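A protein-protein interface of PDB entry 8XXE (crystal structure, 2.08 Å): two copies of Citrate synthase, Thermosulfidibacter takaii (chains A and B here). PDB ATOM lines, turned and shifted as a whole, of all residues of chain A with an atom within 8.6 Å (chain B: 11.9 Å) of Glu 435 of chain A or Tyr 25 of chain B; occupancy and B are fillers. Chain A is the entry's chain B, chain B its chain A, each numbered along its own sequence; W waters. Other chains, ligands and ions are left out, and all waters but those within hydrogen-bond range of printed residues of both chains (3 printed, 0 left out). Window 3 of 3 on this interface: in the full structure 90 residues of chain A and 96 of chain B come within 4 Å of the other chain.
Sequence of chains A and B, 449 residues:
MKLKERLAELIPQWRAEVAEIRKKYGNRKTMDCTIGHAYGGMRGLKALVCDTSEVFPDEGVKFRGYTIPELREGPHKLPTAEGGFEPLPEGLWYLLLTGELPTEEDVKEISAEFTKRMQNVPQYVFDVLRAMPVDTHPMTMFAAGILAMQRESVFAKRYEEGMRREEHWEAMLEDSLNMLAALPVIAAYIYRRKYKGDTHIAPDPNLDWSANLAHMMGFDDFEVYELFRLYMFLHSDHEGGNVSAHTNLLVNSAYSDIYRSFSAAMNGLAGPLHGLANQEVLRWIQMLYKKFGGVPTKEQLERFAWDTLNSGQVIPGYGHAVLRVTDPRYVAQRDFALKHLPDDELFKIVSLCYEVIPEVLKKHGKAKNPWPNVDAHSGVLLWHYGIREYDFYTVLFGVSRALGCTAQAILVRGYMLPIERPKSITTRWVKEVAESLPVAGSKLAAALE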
ATOM      1  N   CYS A  33      -8.442  -1.537 -21.867  1.00  0.00           N
ATOM      2  CA  CYS A  33      -8.427  -1.503 -23.314  1.00  0.00           C
ATOM      3  C   CYS A  33      -8.646  -2.940 -23.778  1.00  0.00           C
ATOM      4  O   CYS A  33      -8.065  -3.870 -23.220  1.00  0.00           O
ATOM      5  CB  CYS A  33      -7.108  -0.868 -23.760  1.00  0.00           C
ATOM      6  SG  CYS A  33      -6.901  -0.714 -25.555  1.00  0.00           S
ATOM      7  N   THR A  34      -9.500  -3.112 -24.783  1.00  0.00           N
ATOM      8  CA  THR A  34      -9.982  -4.410 -25.207  1.00  0.00           C
ATOM      9  C   THR A  34      -9.716  -4.597 -26.700  1.00  0.00           C
ATOM     10  O   THR A  34      -9.351  -3.652 -27.406  1.00  0.00           O
ATOM     11  CB  THR A  34     -11.470  -4.598 -24.882  1.00  0.00           C
ATOM     12  OG1 THR A  34     -12.272  -3.808 -25.757  1.00  0.00           O
ATOM     13  CG2 THR A  34     -11.832  -4.274 -23.444  1.00  0.00           C
ATOM     14  N   ILE A  35      -9.869  -5.843 -27.145  1.00  0.00           N
ATOM     15  CA  ILE A  35      -9.862  -6.226 -28.549  1.00  0.00           C
ATOM     16  C   ILE A  35     -10.993  -5.465 -29.237  1.00  0.00           C
ATOM     17  O   ILE A  35     -10.869  -5.000 -30.371  1.00  0.00           O
ATOM     18  CB  ILE A  35      -9.992  -7.765 -28.693  1.00  0.00           C
ATOM     19  CG1 ILE A  35      -8.747  -8.504 -28.196  1.00  0.00           C
ATOM     20  CG2 ILE A  35     -10.288  -8.192 -30.109  1.00  0.00           C
ATOM     21  CD1 ILE A  35      -7.543  -8.357 -29.115  1.00  0.00           C
ATOM     22  N   GLY A  36     -12.094  -5.340 -28.510  1.00  0.00           N
ATOM     23  CA  GLY A  36     -13.279  -4.670 -28.979  1.00  0.00           C
ATOM     24  C   GLY A  36     -12.998  -3.207 -29.344  1.00  0.00           C
ATOM     25  O   GLY A  36     -13.552  -2.725 -30.330  1.00  0.00           O
ATOM     26  N   HIS A  37     -12.179  -2.512 -28.545  1.00  0.00           N
ATOM     27  CA  HIS A  37     -11.793  -1.131 -28.844  1.00  0.00           C
ATOM     28  C   HIS A  37     -11.037  -1.063 -30.180  1.00  0.00           C
ATOM     29  O   HIS A  37     -11.333  -0.214 -31.025  1.00  0.00           O
ATOM     30  CB  HIS A  37     -10.980  -0.527 -27.702  1.00  0.00           C
ATOM     31  CG  HIS A  37     -11.741  -0.319 -26.432  1.00  0.00           C
ATOM     32  ND1 HIS A  37     -12.788   0.574 -26.307  1.00  0.00           N
ATOM     33  CD2 HIS A  37     -11.582  -0.852 -25.217  1.00  0.00           C
ATOM     34  CE1 HIS A  37     -13.245   0.552 -25.061  1.00  0.00           C
ATOM     35  NE2 HIS A  37     -12.532  -0.308 -24.386  1.00  0.00           N
ATOM     36  N   TYR A  39     -11.071  -3.055 -32.807  1.00  0.00           N
ATOM     37  CA  TYR A  39     -11.847  -3.381 -33.983  1.00  0.00           C
ATOM     38  C   TYR A  39     -13.138  -2.573 -34.013  1.00  0.00           C
ATOM     39  O   TYR A  39     -13.900  -2.696 -34.966  1.00  0.00           O
ATOM     40  CB  TYR A  39     -12.230  -4.868 -34.022  1.00  0.00           C
ATOM     41  CG  TYR A  39     -11.092  -5.772 -34.404  1.00  0.00           C
ATOM     42  CD1 TYR A  39     -10.196  -6.231 -33.457  1.00  0.00           C
ATOM     43  CD2 TYR A  39     -10.889  -6.118 -35.730  1.00  0.00           C
ATOM     44  CE1 TYR A  39      -9.149  -7.058 -33.818  1.00  0.00           C
ATOM     45  CE2 TYR A  39      -9.827  -6.913 -36.106  1.00  0.00           C
ATOM     46  CZ  TYR A  39      -8.963  -7.399 -35.148  1.00  0.00           C
ATOM     47  OH  TYR A  39      -7.911  -8.178 -35.561  1.00  0.00           O
ATOM     48  N   THR A 427      -4.593  -8.929 -36.904  1.00  0.00           N
ATOM     49  CA  THR A 427      -5.576  -9.986 -36.734  1.00  0.00           C
ATOM     50  C   THR A 427      -4.865 -11.316 -36.481  1.00  0.00           C
ATOM     51  O   THR A 427      -5.344 -12.129 -35.695  1.00  0.00           O
ATOM     52  CB  THR A 427      -6.518 -10.022 -37.934  1.00  0.00           C
ATOM     53  OG1 THR A 427      -6.993  -8.684 -38.045  1.00  0.00           O
ATOM     54  CG2 THR A 427      -7.675 -10.988 -37.791  1.00  0.00           C
ATOM     55  N   TRP A 429      -1.945 -11.751 -34.768  1.00  0.00           N
ATOM     56  CA  TRP A 429      -1.686 -11.726 -33.336  1.00  0.00           C
ATOM     57  C   TRP A 429      -2.967 -12.023 -32.555  1.00  0.00           C
ATOM     58  O   TRP A 429      -3.001 -12.939 -31.734  1.00  0.00           O
ATOM     59  CB  TRP A 429      -1.114 -10.377 -32.913  1.00  0.00           C
ATOM     60  CG  TRP A 429      -0.794 -10.243 -31.459  1.00  0.00           C
ATOM     61  CD1 TRP A 429       0.315 -10.721 -30.822  1.00  0.00           C
ATOM     62  CD2 TRP A 429      -1.528  -9.503 -30.465  1.00  0.00           C
ATOM     63  NE1 TRP A 429       0.316 -10.342 -29.509  1.00  0.00           N
ATOM     64  CE2 TRP A 429      -0.796  -9.597 -29.256  1.00  0.00           C
ATOM     65  CE3 TRP A 429      -2.743  -8.806 -30.461  1.00  0.00           C
ATOM     66  CZ2 TRP A 429      -1.234  -9.021 -28.064  1.00  0.00           C
ATOM     67  CZ3 TRP A 429      -3.161  -8.205 -29.291  1.00  0.00           C
ATOM     68  CH2 TRP A 429      -2.415  -8.315 -28.109  1.00  0.00           C
ATOM     69  N   VAL A 430      -4.037 -11.271 -32.837  1.00  0.00           N
ATOM     70  CA  VAL A 430      -5.302 -11.476 -32.140  1.00  0.00           C
ATOM     71  C   VAL A 430      -5.696 -12.961 -32.149  1.00  0.00           C
ATOM     72  O   VAL A 430      -5.963 -13.527 -31.098  1.00  0.00           O
ATOM     73  CB  VAL A 430      -6.435 -10.603 -32.710  1.00  0.00           C
ATOM     74  CG1 VAL A 430      -7.784 -11.010 -32.138  1.00  0.00           C
ATOM     75  CG2 VAL A 430      -6.181  -9.112 -32.486  1.00  0.00           C
ATOM     76  N   LYS A 431      -5.757 -13.586 -33.330  1.00  0.00           N
ATOM     77  CA  LYS A 431      -6.151 -14.982 -33.457  1.00  0.00           C
ATOM     78  C   LYS A 431      -5.242 -15.883 -32.613  1.00  0.00           C
ATOM     79  O   LYS A 431      -5.708 -16.841 -32.012  1.00  0.00           O
ATOM     80  CB  LYS A 431      -6.121 -15.422 -34.921  1.00  0.00           C
ATOM     81  CG  LYS A 431      -7.289 -14.952 -35.766  1.00  0.00           C
ATOM     82  CD  LYS A 431      -7.278 -15.552 -37.154  1.00  0.00           C
ATOM     83  CE  LYS A 431      -7.600 -17.032 -37.150  1.00  0.00           C
ATOM     84  NZ  LYS A 431      -7.389 -17.633 -38.485  1.00  0.00           N
ATOM     85  N   GLU A 432      -3.946 -15.579 -32.565  1.00  0.00           N
ATOM     86  CA  GLU A 432      -3.017 -16.371 -31.779  1.00  0.00           C
ATOM     87  C   GLU A 432      -3.328 -16.248 -30.287  1.00  0.00           C
ATOM     88  O   GLU A 432      -3.299 -17.241 -29.573  1.00  0.00           O
ATOM     89  CB  GLU A 432      -1.569 -15.934 -32.020  1.00  0.00           C
ATOM     90  CG  GLU A 432      -0.557 -16.843 -31.342  1.00  0.00           C
ATOM     91  CD  GLU A 432       0.899 -16.533 -31.641  1.00  0.00           C
ATOM     92  OE1 GLU A 432       1.554 -17.378 -32.290  1.00  0.00           O
ATOM     93  OE2 GLU A 432       1.378 -15.458 -31.216  1.00  0.00           O
ATOM     94  N   VAL A 433      -3.613 -15.028 -29.821  1.00  0.00           N
ATOM     95  CA  VAL A 433      -3.388 -14.669 -28.430  1.00  0.00           C
ATOM     96  C   VAL A 433      -4.704 -14.500 -27.677  1.00  0.00           C
ATOM     97  O   VAL A 433      -4.688 -14.359 -26.468  1.00  0.00           O
ATOM     98  CB  VAL A 433      -2.510 -13.405 -28.382  1.00  0.00           C
ATOM     99  CG1 VAL A 433      -2.885 -12.427 -27.279  1.00  0.00           C
ATOM    100  CG2 VAL A 433      -1.038 -13.772 -28.304  1.00  0.00           C
ATOM    101  N   ALA A 434      -5.842 -14.532 -28.376  1.00  0.00           N
ATOM    102  CA  ALA A 434      -7.097 -14.061 -27.810  1.00  0.00           C
ATOM    103  C   ALA A 434      -7.559 -14.985 -26.681  1.00  0.00           C
ATOM    104  O   ALA A 434      -7.979 -14.508 -25.621  1.00  0.00           O
ATOM    105  CB  ALA A 434      -8.147 -13.954 -28.889  1.00  0.00           C
ATOM    106  N   GLU A 435      -7.466 -16.302 -26.917  1.00  0.00           N
ATOM    107  CA  GLU A 435      -7.741 -17.316 -25.895  1.00  0.00           C
ATOM    108  C   GLU A 435      -6.958 -17.024 -24.617  1.00  0.00           C
ATOM    109  O   GLU A 435      -7.511 -17.124 -23.536  1.00  0.00           O
ATOM    110  CB  GLU A 435      -7.374 -18.725 -26.370  1.00  0.00           C
ATOM    111  CG  GLU A 435      -8.194 -19.228 -27.555  1.00  0.00           C
ATOM    112  CD  GLU A 435      -9.614 -19.691 -27.271  1.00  0.00           C
ATOM    113  OE1 GLU A 435     -10.474 -18.838 -26.996  1.00  0.00           O
ATOM    114  OE2 GLU A 435      -9.860 -20.913 -27.349  1.00  0.00           O
ATOM    115  N   SER A 436      -5.678 -16.657 -24.762  1.00  0.00           N
ATOM    116  CA  SER A 436      -4.769 -16.310 -23.670  1.00  0.00           C
ATOM    117  C   SER A 436      -5.259 -15.128 -22.839  1.00  0.00           C
ATOM    118  O   SER A 436      -4.782 -14.937 -21.730  1.00  0.00           O
ATOM    119  CB  SER A 436      -3.409 -15.936 -24.224  1.00  0.00           C
ATOM    120  OG  SER A 436      -3.018 -16.785 -25.297  1.00  0.00           O
ATOM    121  N   LEU A 437      -6.069 -14.243 -23.443  1.00  0.00           N
ATOM    122  CA  LEU A 437      -6.436 -12.979 -22.827  1.00  0.00           C
ATOM    123  C   LEU A 437      -7.627 -13.171 -21.891  1.00  0.00           C
ATOM    124  O   LEU A 437      -8.595 -13.860 -22.234  1.00  0.00           O
ATOM    125  CB  LEU A 437      -6.811 -11.971 -23.922  1.00  0.00           C
ATOM    126  CG  LEU A 437      -5.751 -10.957 -24.362  1.00  0.00           C
ATOM    127  CD1 LEU A 437      -4.334 -11.499 -24.305  1.00  0.00           C
ATOM    128  CD2 LEU A 437      -6.071 -10.475 -25.771  1.00  0.00           C
ATOM    129  N   PRO A 438      -7.615 -12.502 -20.720  1.00  0.00           N
ATOM    130  CA  PRO A 438      -8.771 -12.481 -19.815  1.00  0.00           C
ATOM    131  C   PRO A 438      -9.958 -11.672 -20.322  1.00  0.00           C
ATOM    132  O   PRO A 438      -9.777 -10.717 -21.078  1.00  0.00           O
ATOM    133  CB  PRO A 438      -8.229 -11.787 -18.560  1.00  0.00           C
ATOM    134  CG  PRO A 438      -7.095 -10.950 -19.071  1.00  0.00           C
ATOM    135  CD  PRO A 438      -6.466 -11.756 -20.187  1.00  0.00           C
ATOM    136  N   VAL A 439     -11.171 -12.053 -19.928  1.00  0.00           N
ATOM    137  CA  VAL A 439     -12.318 -11.203 -20.192  1.00  0.00           C
ATOM    138  C   VAL A 439     -12.202  -9.971 -19.288  1.00  0.00           C
ATOM    139  O   VAL A 439     -11.708 -10.062 -18.171  1.00  0.00           O
ATOM    140  CB  VAL A 439     -13.671 -11.941 -20.095  1.00  0.00           C
ATOM    141  CG1 VAL A 439     -13.689 -13.004 -19.013  1.00  0.00           C
ATOM    142  CG2 VAL A 439     -14.852 -10.981 -19.936  1.00  0.00           C
ATOM    143  N   ALA A 440     -12.501  -8.782 -19.842  1.00  0.00           N
ATOM    144  CA  ALA A 440     -12.367  -7.538 -19.098  1.00  0.00           C
ATOM    145  C   ALA A 440     -13.362  -7.569 -17.940  1.00  0.00           C
ATOM    146  O   ALA A 440     -14.472  -8.068 -18.097  1.00  0.00           O
ATOM    147  CB  ALA A 440     -12.630  -6.350 -20.000  1.00  0.00           C
ATOM    148  N   LEU A 444     -10.274 -13.478 -13.676  1.00  0.00           N
ATOM    149  CA  LEU A 444      -8.962 -13.736 -14.264  1.00  0.00           C
ATOM    150  C   LEU A 444      -8.240 -12.412 -14.575  1.00  0.00           C
ATOM    151  O   LEU A 444      -7.051 -12.271 -14.259  1.00  0.00           O
ATOM    152  CB  LEU A 444      -9.082 -14.622 -15.482  1.00  0.00           C
ATOM    153  N   ALA B  16     -15.868 -12.095 -42.554  1.00  0.00           N
ATOM    154  CA  ALA B  16     -16.550 -13.063 -41.693  1.00  0.00           C
ATOM    155  C   ALA B  16     -15.692 -13.323 -40.463  1.00  0.00           C
ATOM    156  O   ALA B  16     -16.195 -13.346 -39.360  1.00  0.00           O
ATOM    157  CB  ALA B  16     -16.847 -14.356 -42.434  1.00  0.00           C
ATOM    158  N   GLU B  17     -14.379 -13.462 -40.659  1.00  0.00           N
ATOM    159  CA  GLU B  17     -13.466 -13.778 -39.571  1.00  0.00           C
ATOM    160  C   GLU B  17     -13.412 -12.634 -38.567  1.00  0.00           C
ATOM    161  O   GLU B  17     -13.194 -12.848 -37.373  1.00  0.00           O
ATOM    162  CB  GLU B  17     -12.074 -14.013 -40.145  1.00  0.00           C
ATOM    163  CG  GLU B  17     -11.222 -14.958 -39.334  1.00  0.00           C
ATOM    164  CD  GLU B  17      -9.869 -15.181 -39.985  1.00  0.00           C
ATOM    165  OE1 GLU B  17      -8.944 -14.403 -39.693  1.00  0.00           O
ATOM    166  OE2 GLU B  17      -9.773 -16.079 -40.839  1.00  0.00           O
ATOM    167  N   VAL B  18     -13.565 -11.400 -39.069  1.00  0.00           N
ATOM    168  CA  VAL B  18     -13.430 -10.243 -38.204  1.00  0.00           C
ATOM    169  C   VAL B  18     -14.710 -10.114 -37.385  1.00  0.00           C
ATOM    170  O   VAL B  18     -14.638  -9.796 -36.210  1.00  0.00           O
ATOM    171  CB  VAL B  18     -13.086  -8.958 -38.995  1.00  0.00           C
ATOM    172  CG1 VAL B  18     -13.423  -7.685 -38.230  1.00  0.00           C
ATOM    173  CG2 VAL B  18     -11.622  -8.948 -39.414  1.00  0.00           C
ATOM    174  N   ALA B  19     -15.869 -10.320 -38.016  1.00  0.00           N
ATOM    175  CA  ALA B  19     -17.137 -10.320 -37.301  1.00  0.00           C
ATOM    176  C   ALA B  19     -17.117 -11.371 -36.190  1.00  0.00           C
ATOM    177  O   ALA B  19     -17.588 -11.109 -35.082  1.00  0.00           O
ATOM    178  CB  ALA B  19     -18.277 -10.568 -38.260  1.00  0.00           C
ATOM    179  N   GLU B  20     -16.507 -12.532 -36.475  1.00  0.00           N
ATOM    180  CA  GLU B  20     -16.417 -13.619 -35.502  1.00  0.00           C
ATOM    181  C   GLU B  20     -15.578 -13.163 -34.317  1.00  0.00           C
ATOM    182  O   GLU B  20     -16.033 -13.242 -33.182  1.00  0.00           O
ATOM    183  CB  GLU B  20     -15.899 -14.901 -36.164  1.00  0.00           C
ATOM    184  CG  GLU B  20     -15.197 -15.874 -35.223  1.00  0.00           C
ATOM    185  CD  GLU B  20     -16.102 -16.783 -34.409  1.00  0.00           C
ATOM    186  OE1 GLU B  20     -16.872 -16.265 -33.564  1.00  0.00           O
ATOM    187  OE2 GLU B  20     -16.017 -18.014 -34.616  1.00  0.00           O
ATOM    188  N   ILE B  21     -14.378 -12.634 -34.588  1.00  0.00           N
ATOM    189  CA  ILE B  21     -13.471 -12.126 -33.566  1.00  0.00           C
ATOM    190  C   ILE B  21     -14.130 -11.038 -32.718  1.00  0.00           C
ATOM    191  O   ILE B  21     -13.908 -10.984 -31.522  1.00  0.00           O
ATOM    192  CB  ILE B  21     -12.174 -11.615 -34.223  1.00  0.00           C
ATOM    193  CG1 ILE B  21     -11.327 -12.777 -34.736  1.00  0.00           C
ATOM    194  CG2 ILE B  21     -11.389 -10.708 -33.287  1.00  0.00           C
ATOM    195  CD1 ILE B  21     -10.390 -12.398 -35.853  1.00  0.00           C
ATOM    196  N   ARG B  22     -14.940 -10.161 -33.322  1.00  0.00           N
ATOM    197  CA  ARG B  22     -15.559  -9.087 -32.564  1.00  0.00           C
ATOM    198  C   ARG B  22     -16.636  -9.644 -31.621  1.00  0.00           C
ATOM    199  O   ARG B  22     -16.772  -9.156 -30.504  1.00  0.00           O
ATOM    200  CB  ARG B  22     -16.125  -8.011 -33.505  1.00  0.00           C
ATOM    201  CG  ARG B  22     -15.049  -7.271 -34.299  1.00  0.00           C
ATOM    202  CD  ARG B  22     -15.612  -6.184 -35.193  1.00  0.00           C
ATOM    203  NE  ARG B  22     -16.248  -5.107 -34.462  1.00  0.00           N
ATOM    204  CZ  ARG B  22     -17.116  -4.268 -35.005  1.00  0.00           C
ATOM    205  NH1 ARG B  22     -17.525  -4.472 -36.241  1.00  0.00           N
ATOM    206  NH2 ARG B  22     -17.577  -3.240 -34.322  1.00  0.00           N
ATOM    207  N   LYS B  23     -17.449 -10.591 -32.109  1.00  0.00           N
ATOM    208  CA  LYS B  23     -18.463 -11.252 -31.298  1.00  0.00           C
ATOM    209  C   LYS B  23     -17.781 -12.069 -30.198  1.00  0.00           C
ATOM    210  O   LYS B  23     -17.969 -11.827 -29.010  1.00  0.00           O
ATOM    211  CB  LYS B  23     -19.320 -12.142 -32.198  1.00  0.00           C
ATOM    212  CG  LYS B  23     -20.627 -12.626 -31.595  1.00  0.00           C
ATOM    213  CD  LYS B  23     -21.624 -13.080 -32.651  1.00  0.00           C
ATOM    214  CE  LYS B  23     -23.006 -12.480 -32.464  1.00  0.00           C
ATOM    215  NZ  LYS B  23     -23.744 -12.400 -33.746  1.00  0.00           N
ATOM    216  N   LYS B  24     -16.908 -12.993 -30.594  1.00  0.00           N
ATOM    217  CA  LYS B  24     -16.332 -13.932 -29.648  1.00  0.00           C
ATOM    218  C   LYS B  24     -15.371 -13.275 -28.653  1.00  0.00           C
ATOM    219  O   LYS B  24     -15.384 -13.654 -27.489  1.00  0.00           O
ATOM    220  CB  LYS B  24     -15.657 -15.080 -30.400  1.00  0.00           C
ATOM    221  CG  LYS B  24     -14.837 -16.009 -29.517  1.00  0.00           C
ATOM    222  CD  LYS B  24     -14.262 -17.200 -30.248  1.00  0.00           C
ATOM    223  CE  LYS B  24     -15.293 -18.239 -30.617  1.00  0.00           C
ATOM    224  NZ  LYS B  24     -14.704 -19.597 -30.539  1.00  0.00           N
ATOM    225  N   TYR B  25     -14.504 -12.338 -29.079  1.00  0.00           N
ATOM    226  CA  TYR B  25     -13.370 -11.906 -28.253  1.00  0.00           C
ATOM    227  C   TYR B  25     -13.344 -10.396 -27.969  1.00  0.00           C
ATOM    228  O   TYR B  25     -12.358  -9.866 -27.423  1.00  0.00           O
ATOM    229  CB  TYR B  25     -12.055 -12.271 -28.938  1.00  0.00           C
ATOM    230  CG  TYR B  25     -11.777 -13.743 -29.087  1.00  0.00           C
ATOM    231  CD1 TYR B  25     -11.635 -14.554 -27.973  1.00  0.00           C
ATOM    232  CD2 TYR B  25     -11.622 -14.327 -30.337  1.00  0.00           C
ATOM    233  CE1 TYR B  25     -11.340 -15.904 -28.096  1.00  0.00           C
ATOM    234  CE2 TYR B  25     -11.334 -15.676 -30.481  1.00  0.00           C
ATOM    235  CZ  TYR B  25     -11.194 -16.467 -29.351  1.00  0.00           C
ATOM    236  OH  TYR B  25     -10.928 -17.814 -29.451  1.00  0.00           O
ATOM    237  N   GLY B  26     -14.432  -9.697 -28.285  1.00  0.00           N
ATOM    238  CA  GLY B  26     -14.457  -8.244 -28.163  1.00  0.00           C
ATOM    239  C   GLY B  26     -14.119  -7.774 -26.755  1.00  0.00           C
ATOM    240  O   GLY B  26     -13.504  -6.728 -26.562  1.00  0.00           O
ATOM    241  N   ASN B  27     -14.530  -8.566 -25.756  1.00  0.00           N
ATOM    242  CA  ASN B  27     -14.437  -8.157 -24.362  1.00  0.00           C
ATOM    243  C   ASN B  27     -13.096  -8.558 -23.755  1.00  0.00           C
ATOM    244  O   ASN B  27     -12.834  -8.305 -22.584  1.00  0.00           O
ATOM    245  CB  ASN B  27     -15.614  -8.724 -23.554  1.00  0.00           C
ATOM    246  CG  ASN B  27     -15.691 -10.240 -23.586  1.00  0.00           C
ATOM    247  OD1 ASN B  27     -14.681 -10.939 -23.722  1.00  0.00           O
ATOM    248  ND2 ASN B  27     -16.892 -10.760 -23.421  1.00  0.00           N
ATOM    249  N   ARG B  28     -12.227  -9.192 -24.539  1.00  0.00           N
ATOM    250  CA  ARG B  28     -10.922  -9.570 -24.026  1.00  0.00           C
ATOM    251  C   ARG B  28     -10.072  -8.329 -23.814  1.00  0.00           C
ATOM    252  O   ARG B  28      -9.992  -7.472 -24.687  1.00  0.00           O
ATOM    253  CB  ARG B  28     -10.209 -10.512 -25.003  1.00  0.00           C
ATOM    254  CG  ARG B  28     -10.864 -11.881 -25.125  1.00  0.00           C
ATOM    255  CD  ARG B  28     -10.603 -12.693 -23.864  1.00  0.00           C
ATOM    256  NE  ARG B  28     -10.966 -14.101 -23.982  1.00  0.00           N
ATOM    257  CZ  ARG B  28     -12.183 -14.540 -24.262  1.00  0.00           C
ATOM    258  NH1 ARG B  28     -13.181 -13.681 -24.429  1.00  0.00           N
ATOM    259  NH2 ARG B  28     -12.397 -15.841 -24.376  1.00  0.00           N
ATOM    260  N   LYS B  29      -9.380  -8.279 -22.680  1.00  0.00           N
ATOM    261  CA  LYS B  29      -8.533  -7.155 -22.345  1.00  0.00           C
ATOM    262  C   LYS B  29      -7.131  -7.326 -22.904  1.00  0.00           C
ATOM    263  O   LYS B  29      -6.577  -8.400 -22.760  1.00  0.00           O
ATOM    264  CB  LYS B  29      -8.442  -7.055 -20.829  1.00  0.00           C
ATOM    265  CG  LYS B  29      -7.312  -6.193 -20.333  1.00  0.00           C
ATOM    266  CD  LYS B  29      -7.420  -5.952 -18.878  1.00  0.00           C
ATOM    267  CE  LYS B  29      -6.219  -5.209 -18.362  1.00  0.00           C
ATOM    268  NZ  LYS B  29      -6.458  -4.802 -16.968  1.00  0.00           N
ATOM    269  N   THR B  30      -6.555  -6.245 -23.470  1.00  0.00           N
ATOM    270  CA  THR B  30      -5.187  -6.247 -23.971  1.00  0.00           C
ATOM    271  C   THR B  30      -4.237  -5.479 -23.059  1.00  0.00           C
ATOM    272  O   THR B  30      -3.045  -5.730 -23.079  1.00  0.00           O
ATOM    273  CB  THR B  30      -5.084  -5.620 -25.378  1.00  0.00           C
ATOM    274  OG1 THR B  30      -5.584  -4.279 -25.318  1.00  0.00           O
ATOM    275  CG2 THR B  30      -5.880  -6.377 -26.411  1.00  0.00           C
ATOM    276  N   MET B  31      -4.724  -4.487 -22.310  1.00  0.00           N
ATOM    277  CA  MET B  31      -3.853  -3.689 -21.462  1.00  0.00           C
ATOM    278  C   MET B  31      -4.728  -2.688 -20.709  1.00  0.00           C
ATOM    279  O   MET B  31      -5.939  -2.628 -20.929  1.00  0.00           O
ATOM    280  CB  MET B  31      -2.803  -2.920 -22.278  1.00  0.00           C
ATOM    281  CG  MET B  31      -3.427  -2.070 -23.418  1.00  0.00           C
ATOM    282  SD  MET B  31      -2.224  -1.234 -24.525  1.00  0.00           S
ATOM    283  CE  MET B  31      -1.278  -0.220 -23.399  1.00  0.00           C
ATOM    284  N   LYS B  46      -2.963   0.039 -27.577  1.00  0.00           N
ATOM    285  CA  LYS B  46      -3.368  -0.868 -28.657  1.00  0.00           C
ATOM    286  C   LYS B  46      -4.783  -0.542 -29.150  1.00  0.00           C
ATOM    287  O   LYS B  46      -5.751  -1.243 -28.849  1.00  0.00           O
ATOM    288  CB  LYS B  46      -3.242  -2.321 -28.177  1.00  0.00           C
ATOM    289  CG  LYS B  46      -1.816  -2.810 -27.928  1.00  0.00           C
ATOM    290  CD  LYS B  46      -1.781  -4.232 -27.400  1.00  0.00           C
ATOM    291  CE  LYS B  46      -0.400  -4.845 -27.400  1.00  0.00           C
ATOM    292  NZ  LYS B  46       0.486  -4.160 -26.438  1.00  0.00           N
ATOM    293  N   VAL B  49      -6.310  -1.364 -35.604  1.00  0.00           N
ATOM    294  CA  VAL B  49      -6.023  -2.580 -36.353  1.00  0.00           C
ATOM    295  C   VAL B  49      -5.256  -2.212 -37.624  1.00  0.00           C
ATOM    296  O   VAL B  49      -5.667  -1.297 -38.339  1.00  0.00           O
ATOM    297  CB  VAL B  49      -7.321  -3.314 -36.747  1.00  0.00           C
ATOM    298  CG1 VAL B  49      -7.049  -4.503 -37.659  1.00  0.00           C
ATOM    299  CG2 VAL B  49      -8.107  -3.766 -35.532  1.00  0.00           C
HETATM  300  O   HOH W   1      -6.649  -3.563 -27.697  1.00  0.00           O
HETATM  301  O   HOH W   2     -15.200  -4.380 -31.893  1.00  0.00           O
HETATM  302  O   HOH W   3     -14.678  -4.020 -25.422  1.00  0.00           O
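OD1 of Asn 27 of chain B is in hydrogen-bond range of NH1 of Arg 28 of chain B. OH of Tyr 39 of chain A lies within hydrogen-bond range of OG1 of Thr 427 of chain A, at 2.7 Å.
OE2 of Glu 17 of chain B is in salt-bridge range of NZ of Lys 431 of chain A (3.7 Å). The side-chain carboxylate of Glu 435 of chain A sits at hydrogen-bond distance from the side-chain hydroxyl of Tyr 25 of chain B. O of Gly 26 of chain B is in hydrogen-bond range of OG1 of Thr 34 of chain A, 3.3 Å away. The backbone carbonyl oxygen (O) of Gly 26 of chain B sits at hydrogen-bond distance from the backbone NH (N) of Gly 36 of chain A, at 2.8 Å. The backbone carbonyl oxygen of Asn 27 of chain B sits at hydrogen-bond distance from the backbone NH of Ala 440 of chain A, at 2.8 Å. The guanidinium group (NE) of Arg 28 of chain B lies within hydrogen-bond range of the backbone carbonyl oxygen (O) of Ala 434 of chain A, 3.4 Å away. The backbone carbonyl oxygen (O) of Leu 437 of chain A lies close to the guanidinium group (NE) of Arg 28 of chain B (3.0 Å). The backbone NH (N) of Thr 30 of chain B lies within hydrogen-bond range of the backbone carbonyl oxygen (O) of Cys 33 of chain A (2.8 Å). The backbone NH of Cys 33 of chain A is in hydrogen-bond range of the backbone carbonyl oxygen of Met 31 of chain B, at 2.9 Å.
Tyr 25 of chain B touches Ile 35 of chain A. O of Gly 26 of chain B touches N of Ile 35 of chain A (3.8 Å). Ile 21 of chain B touches Thr 427 of chain A. Val 439 of chain A touches Asn 27 of chain B (C to O, 3.7 Å).
Water W3 bridges OG1 of Thr 34 of chain A (2.4 Å) and O of Gly 26 of chain B (3.2 Å). Water W2 bridges the backbone carbonyl oxygen (O) of Gly 36 of chain A (2.8 Å) and the guanidinium group (NE) of Arg 22 of chain B (2.9 Å).
Tyr 25 of chain B touches just these residues of chain A: Ile 35, Ala 434 and Glu 435. No residue of chain B comes within 4 Å of Ser 436 of chain A. Pro 438 of chain A touches two residues of chain B. Of the printed residues of chain B, Val 439 of chain A touches Asn 27 (3.7 Å). Printed residues of chain A within 4 Å of Lys 46 of chain B: Cys 33 (3.5 Å). The nearest printed residue of chain A that does not touch Met 31 of chain B is Thr 34 of chain A (5.3 Å).
Of the 20 printed residues of chain A, 14 touch a printed residue of chain B. Hydrophobic or aromatic side chains of chain A that line the printed part of chain B: Ile 35, Tyr 39, Val 430, Ala 434, Leu 437, Val 439 and Ala 440.
No position is printed for both chains. Of the 26 pairs that touch across the chains among the printed residues, none has its exchanged pair printed and touching as well.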
